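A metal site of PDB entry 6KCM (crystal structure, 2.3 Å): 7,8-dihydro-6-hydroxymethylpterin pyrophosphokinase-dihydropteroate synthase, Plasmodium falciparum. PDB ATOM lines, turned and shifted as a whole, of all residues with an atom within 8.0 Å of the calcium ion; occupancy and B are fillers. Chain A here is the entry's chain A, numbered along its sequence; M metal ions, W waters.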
ATOM      1  N   LEU A  38      22.631  13.651   2.720  1.00  0.00           N
ATOM      2  CA  LEU A  38      22.253  14.891   1.997  1.00  0.00           C
ATOM      3  C   LEU A  38      22.460  14.785   0.493  1.00  0.00           C
ATOM      4  O   LEU A  38      21.559  15.098  -0.296  1.00  0.00           O
ATOM      5  CB  LEU A  38      23.019  16.109   2.523  1.00  0.00           C
ATOM      6  CG  LEU A  38      22.723  16.625   3.927  1.00  0.00           C
ATOM      7  CD1 LEU A  38      23.495  17.897   4.208  1.00  0.00           C
ATOM      8  CD2 LEU A  38      21.225  16.858   4.096  1.00  0.00           C
ATOM      9  N   HIS A  39      23.639  14.306   0.089  1.00  0.00           N
ATOM     10  CA  HIS A  39      23.924  14.151  -1.354  1.00  0.00           C
ATOM     11  C   HIS A  39      22.957  13.195  -2.002  1.00  0.00           C
ATOM     12  O   HIS A  39      22.409  13.506  -3.051  1.00  0.00           O
ATOM     13  CB  HIS A  39      25.355  13.698  -1.585  1.00  0.00           C
ATOM     14  CG  HIS A  39      26.385  14.756  -1.286  1.00  0.00           C
ATOM     15  ND1 HIS A  39      26.371  15.975  -1.892  1.00  0.00           N
ATOM     16  CD2 HIS A  39      27.467  14.766  -0.409  1.00  0.00           C
ATOM     17  CE1 HIS A  39      27.398  16.709  -1.426  1.00  0.00           C
ATOM     18  NE2 HIS A  39      28.066  15.972  -0.512  1.00  0.00           N
ATOM     19  N   LEU A  40      22.713  12.055  -1.348  1.00  0.00           N
ATOM     20  CA  LEU A  40      21.791  11.056  -1.891  1.00  0.00           C
ATOM     21  C   LEU A  40      20.355  11.580  -1.950  1.00  0.00           C
ATOM     22  O   LEU A  40      19.630  11.243  -2.889  1.00  0.00           O
ATOM     23  CB  LEU A  40      21.882   9.722  -1.140  1.00  0.00           C
ATOM     24  CG  LEU A  40      23.294   9.099  -1.347  1.00  0.00           C
ATOM     25  CD1 LEU A  40      23.484   7.810  -0.556  1.00  0.00           C
ATOM     26  CD2 LEU A  40      23.612   8.884  -2.833  1.00  0.00           C
ATOM     27  N   VAL A  41      19.984  12.408  -0.976  1.00  0.00           N
ATOM     28  CA  VAL A  41      18.704  13.124  -0.993  1.00  0.00           C
ATOM     29  C   VAL A  41      18.630  14.131  -2.146  1.00  0.00           C
ATOM     30  O   VAL A  41      17.571  14.260  -2.752  1.00  0.00           O
ATOM     31  CB  VAL A  41      18.412  13.866   0.326  1.00  0.00           C
ATOM     32  CG1 VAL A  41      17.168  14.734   0.218  1.00  0.00           C
ATOM     33  CG2 VAL A  41      18.303  12.876   1.485  1.00  0.00           C
ATOM     34  N   GLU A  42      19.739  14.847  -2.435  1.00  0.00           N
ATOM     35  CA  GLU A  42      19.746  15.803  -3.551  1.00  0.00           C
ATOM     36  C   GLU A  42      19.650  15.067  -4.865  1.00  0.00           C
ATOM     37  O   GLU A  42      19.063  15.571  -5.826  1.00  0.00           O
ATOM     38  CB  GLU A  42      21.023  16.667  -3.609  1.00  0.00           C
ATOM     39  CG  GLU A  42      20.910  18.046  -3.000  1.00  0.00           C
ATOM     40  CD  GLU A  42      19.998  19.023  -3.727  1.00  0.00           C
ATOM     41  OE1 GLU A  42      19.519  18.713  -4.845  1.00  0.00           O
ATOM     42  OE2 GLU A  42      19.774  20.133  -3.158  1.00  0.00           O
ATOM     43  N   LYS A  43      20.258  13.892  -4.909  1.00  0.00           N
ATOM     44  CA  LYS A  43      20.300  13.133  -6.155  1.00  0.00           C
ATOM     45  C   LYS A  43      18.982  12.404  -6.407  1.00  0.00           C
ATOM     46  O   LYS A  43      18.491  12.417  -7.524  1.00  0.00           O
ATOM     47  CB  LYS A  43      21.443  12.124  -6.113  1.00  0.00           C
ATOM     48  CG  LYS A  43      21.678  11.367  -7.414  1.00  0.00           C
ATOM     49  CD  LYS A  43      22.734  10.287  -7.127  1.00  0.00           C
ATOM     50  CE  LYS A  43      23.155   9.521  -8.376  1.00  0.00           C
ATOM     51  NZ  LYS A  43      23.994  10.306  -9.324  1.00  0.00           N
ATOM     52  N   TYR A  44      18.432  11.776  -5.374  1.00  0.00           N
ATOM     53  CA  TYR A  44      17.328  10.849  -5.614  1.00  0.00           C
ATOM     54  C   TYR A  44      15.933  11.326  -5.260  1.00  0.00           C
ATOM     55  O   TYR A  44      14.965  10.698  -5.675  1.00  0.00           O
ATOM     56  CB  TYR A  44      17.579   9.501  -4.928  1.00  0.00           C
ATOM     57  CG  TYR A  44      18.711   8.686  -5.512  1.00  0.00           C
ATOM     58  CD1 TYR A  44      18.854   8.527  -6.902  1.00  0.00           C
ATOM     59  CD2 TYR A  44      19.625   8.041  -4.673  1.00  0.00           C
ATOM     60  CE1 TYR A  44      19.883   7.769  -7.428  1.00  0.00           C
ATOM     61  CE2 TYR A  44      20.667   7.280  -5.192  1.00  0.00           C
ATOM     62  CZ  TYR A  44      20.781   7.148  -6.565  1.00  0.00           C
ATOM     63  OH  TYR A  44      21.808   6.388  -7.058  1.00  0.00           O
ATOM     64  N   LEU A  45      15.824  12.408  -4.498  1.00  0.00           N
ATOM     65  CA  LEU A  45      14.522  12.870  -4.006  1.00  0.00           C
ATOM     66  C   LEU A  45      14.034  14.252  -4.502  1.00  0.00           C
ATOM     67  O   LEU A  45      12.841  14.517  -4.480  1.00  0.00           O
ATOM     68  CB  LEU A  45      14.471  12.784  -2.472  1.00  0.00           C
ATOM     69  CG  LEU A  45      14.593  11.369  -1.871  1.00  0.00           C
ATOM     70  CD1 LEU A  45      14.741  11.405  -0.345  1.00  0.00           C
ATOM     71  CD2 LEU A  45      13.393  10.505  -2.261  1.00  0.00           C
ATOM     72  N   GLY A  46      14.928  15.128  -4.951  1.00  0.00           N
ATOM     73  CA  GLY A  46      14.464  16.491  -5.295  1.00  0.00           C
ATOM     74  C   GLY A  46      15.499  17.560  -4.970  1.00  0.00           C
ATOM     75  O   GLY A  46      16.682  17.310  -5.083  1.00  0.00           O
ATOM     76  N   LYS A  47      15.048  18.752  -4.580  1.00  0.00           N
ATOM     77  CA  LYS A  47      15.957  19.836  -4.220  1.00  0.00           C
ATOM     78  C   LYS A  47      15.918  20.176  -2.704  1.00  0.00           C
ATOM     79  O   LYS A  47      14.831  20.333  -2.121  1.00  0.00           O
ATOM     80  CB  LYS A  47      15.644  21.078  -5.067  1.00  0.00           C
ATOM     81  CG  LYS A  47      16.647  22.221  -4.926  1.00  0.00           C
ATOM     82  CD  LYS A  47      16.161  23.498  -5.619  1.00  0.00           C
ATOM     83  CE  LYS A  47      17.163  24.673  -5.476  1.00  0.00           C
ATOM     84  NZ  LYS A  47      18.598  24.313  -5.670  1.00  0.00           N
ATOM     85  N   ILE A  48      17.095  20.301  -2.077  1.00  0.00           N
ATOM     86  CA  ILE A  48      17.180  20.766  -0.672  1.00  0.00           C
ATOM     87  C   ILE A  48      17.072  22.291  -0.624  1.00  0.00           C
ATOM     88  O   ILE A  48      17.890  22.999  -1.213  1.00  0.00           O
ATOM     89  CB  ILE A  48      18.519  20.310  -0.011  1.00  0.00           C
ATOM     90  CG1 ILE A  48      18.562  18.791   0.070  1.00  0.00           C
ATOM     91  CG2 ILE A  48      18.727  20.936   1.376  1.00  0.00           C
ATOM     92  CD1 ILE A  48      19.863  18.227   0.630  1.00  0.00           C
ATOM     93  N   SER A  95      19.762   9.015 -11.145  1.00  0.00           N
ATOM     94  CA  SER A  95      18.367   9.438 -11.034  1.00  0.00           C
ATOM     95  C   SER A  95      17.770   9.557 -12.436  1.00  0.00           C
ATOM     96  O   SER A  95      18.497   9.747 -13.390  1.00  0.00           O
ATOM     97  CB  SER A  95      18.300  10.812 -10.361  1.00  0.00           C
ATOM     98  OG  SER A  95      16.977  11.295 -10.331  1.00  0.00           O
ATOM     99  N   TYR A  97      15.631  11.930 -12.729  1.00  0.00           N
ATOM    100  CA  TYR A  97      15.214  13.317 -12.621  1.00  0.00           C
ATOM    101  C   TYR A  97      16.382  14.287 -12.688  1.00  0.00           C
ATOM    102  O   TYR A  97      17.482  13.976 -12.254  1.00  0.00           O
ATOM    103  CB  TYR A  97      14.397  13.515 -11.356  1.00  0.00           C
ATOM    104  CG  TYR A  97      12.999  12.969 -11.516  1.00  0.00           C
ATOM    105  CD1 TYR A  97      12.776  11.591 -11.460  1.00  0.00           C
ATOM    106  CD2 TYR A  97      11.916  13.809 -11.739  1.00  0.00           C
ATOM    107  CE1 TYR A  97      11.499  11.073 -11.626  1.00  0.00           C
ATOM    108  CE2 TYR A  97      10.641  13.288 -11.896  1.00  0.00           C
ATOM    109  CZ  TYR A  97      10.449  11.917 -11.833  1.00  0.00           C
ATOM    110  OH  TYR A  97       9.223  11.360 -11.960  1.00  0.00           O
ATOM    111  N   GLU A  98      16.105  15.465 -13.239  1.00  0.00           N
ATOM    112  CA  GLU A  98      17.132  16.486 -13.473  1.00  0.00           C
ATOM    113  C   GLU A  98      17.706  17.106 -12.196  1.00  0.00           C
ATOM    114  O   GLU A  98      16.969  17.317 -11.220  1.00  0.00           O
ATOM    115  CB  GLU A  98      16.515  17.652 -14.225  1.00  0.00           C
ATOM    116  CG  GLU A  98      16.262  17.439 -15.699  1.00  0.00           C
ATOM    117  CD  GLU A  98      15.580  18.652 -16.317  1.00  0.00           C
ATOM    118  OE1 GLU A  98      14.671  19.235 -15.691  1.00  0.00           O
ATOM    119  OE2 GLU A  98      15.967  19.022 -17.439  1.00  0.00           O
ATOM    120  N   GLU A  99      18.997  17.443 -12.228  1.00  0.00           N
ATOM    121  CA  GLU A  99      19.582  18.333 -11.231  1.00  0.00           C
ATOM    122  C   GLU A  99      19.804  19.752 -11.800  1.00  0.00           C
ATOM    123  O   GLU A  99      20.735  19.945 -12.569  1.00  0.00           O
ATOM    124  CB  GLU A  99      20.889  17.745 -10.693  1.00  0.00           C
ATOM    125  CG  GLU A  99      21.444  18.535  -9.519  1.00  0.00           C
ATOM    126  CD  GLU A  99      20.547  18.452  -8.294  1.00  0.00           C
ATOM    127  OE1 GLU A  99      19.713  19.400  -8.057  1.00  0.00           O
ATOM    128  OE2 GLU A  99      20.645  17.410  -7.602  1.00  0.00           O
ATOM    129  N   ASN A 100      18.972  20.726 -11.409  1.00  0.00           N
ATOM    130  CA  ASN A 100      19.122  22.141 -11.797  1.00  0.00           C
ATOM    131  C   ASN A 100      19.781  23.027 -10.742  1.00  0.00           C
ATOM    132  O   ASN A 100      19.254  23.204  -9.652  1.00  0.00           O
ATOM    133  CB  ASN A 100      17.764  22.773 -12.140  1.00  0.00           C
ATOM    134  CG  ASN A 100      17.132  22.161 -13.401  1.00  0.00           C
ATOM    135  OD1 ASN A 100      17.747  22.096 -14.487  1.00  0.00           O
ATOM    136  ND2 ASN A 100      15.911  21.711 -13.254  1.00  0.00           N
ATOM    137  N   LYS A 101      20.898  23.652 -11.102  1.00  0.00           N
ATOM    138  CA  LYS A 101      21.671  24.433 -10.149  1.00  0.00           C
ATOM    139  C   LYS A 101      21.445  25.909 -10.182  1.00  0.00           C
ATOM    140  O   LYS A 101      22.042  26.614  -9.395  1.00  0.00           O
ATOM    141  CB  LYS A 101      23.177  24.172 -10.331  1.00  0.00           C
ATOM    142  CG  LYS A 101      23.621  22.771  -9.943  1.00  0.00           C
ATOM    143  CD  LYS A 101      25.109  22.566 -10.153  1.00  0.00           C
ATOM    144  CE  LYS A 101      25.438  21.076 -10.073  1.00  0.00           C
ATOM    145  NZ  LYS A 101      26.772  20.718 -10.640  1.00  0.00           N
ATOM    146  N   VAL A 170      12.950  19.355   1.576  1.00  0.00           N
ATOM    147  CA  VAL A 170      13.187  18.872   0.232  1.00  0.00           C
ATOM    148  C   VAL A 170      11.964  19.194  -0.622  1.00  0.00           C
ATOM    149  O   VAL A 170      10.827  18.828  -0.262  1.00  0.00           O
ATOM    150  CB  VAL A 170      13.344  17.339   0.225  1.00  0.00           C
ATOM    151  CG1 VAL A 170      13.685  16.805  -1.165  1.00  0.00           C
ATOM    152  CG2 VAL A 170      14.372  16.908   1.245  1.00  0.00           C
ATOM    153  N   LYS A 171      12.186  19.892  -1.737  1.00  0.00           N
ATOM    154  CA  LYS A 171      11.158  20.063  -2.753  1.00  0.00           C
ATOM    155  C   LYS A 171      11.301  18.808  -3.627  1.00  0.00           C
ATOM    156  O   LYS A 171      12.322  18.619  -4.284  1.00  0.00           O
ATOM    157  CB  LYS A 171      11.391  21.358  -3.529  1.00  0.00           C
ATOM    158  CG  LYS A 171      10.504  21.648  -4.728  1.00  0.00           C
ATOM    159  CD  LYS A 171      11.128  22.736  -5.625  1.00  0.00           C
ATOM    160  CE  LYS A 171      10.462  24.103  -5.489  1.00  0.00           C
ATOM    161  NZ  LYS A 171      11.283  25.271  -5.935  1.00  0.00           N
ATOM    162  N   PHE A 173      10.116  15.592  -6.267  1.00  0.00           N
ATOM    163  CA  PHE A 173       9.333  15.089  -7.403  1.00  0.00           C
ATOM    164  C   PHE A 173       8.623  13.750  -7.085  1.00  0.00           C
ATOM    165  O   PHE A 173       7.831  13.245  -7.889  1.00  0.00           O
ATOM    166  CB  PHE A 173      10.212  14.917  -8.661  1.00  0.00           C
ATOM    167  CG  PHE A 173      11.577  14.349  -8.371  1.00  0.00           C
ATOM    168  CD1 PHE A 173      11.760  12.979  -8.142  1.00  0.00           C
ATOM    169  CD2 PHE A 173      12.713  15.187  -8.374  1.00  0.00           C
ATOM    170  CE1 PHE A 173      13.011  12.455  -7.896  1.00  0.00           C
ATOM    171  CE2 PHE A 173      13.966  14.669  -8.115  1.00  0.00           C
ATOM    172  CZ  PHE A 173      14.122  13.294  -7.870  1.00  0.00           C
ATOM    173  N   LYS A 518      29.125  23.420  -3.678  1.00  0.00           N
ATOM    174  CA  LYS A 518      28.610  22.049  -3.738  1.00  0.00           C
ATOM    175  C   LYS A 518      29.234  21.245  -4.862  1.00  0.00           C
ATOM    176  O   LYS A 518      29.422  21.762  -5.977  1.00  0.00           O
ATOM    177  CB  LYS A 518      27.102  22.056  -3.979  1.00  0.00           C
ATOM    178  CG  LYS A 518      26.304  22.727  -2.880  1.00  0.00           C
ATOM    179  CD  LYS A 518      25.129  23.466  -3.488  1.00  0.00           C
ATOM    180  CE  LYS A 518      23.922  22.571  -3.635  1.00  0.00           C
ATOM    181  NZ  LYS A 518      22.713  23.404  -3.821  1.00  0.00           N
HETATM  182 CA    CA M   1      18.355  17.539  -6.717  1.00  0.00          CA
HETATM  183  O   HOH W   1      16.987  19.041  -7.190  1.00  0.00           O
HETATM  184  O   HOH W   2      17.564  16.804  -8.630  1.00  0.00           O
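OE2 of Glu 42 lies within hydrogen-bond range of N of Ile 48 (2.9 Å).
Of the 21 residues printed, 3 come within 4 Å of the calcium ion.
The nearest printed residue that does not touch the calcium ion is Lys 47 (4.1 Å).
Water W1 binds the calcium ion, 2.1 Å away.
Water W2 is bound to the calcium ion (2.2 Å).
The calcium ion is bound by the backbone carbonyl oxygen (O) of Glu 42 (2.3 Å).
The calcium ion is bound by O of Gly 46, 2.3 Å away.
The calcium ion is bound by the side-chain carboxylate (OE2) of Glu 99, at 2.5 Å.
The side-chain carboxylate (OE1) of Glu 42 is bound to the calcium ion.
The calcium ion is bound by OE1 of Glu 99 (2.7 Å).
The calcium ion has seven donor atoms within binding distance.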
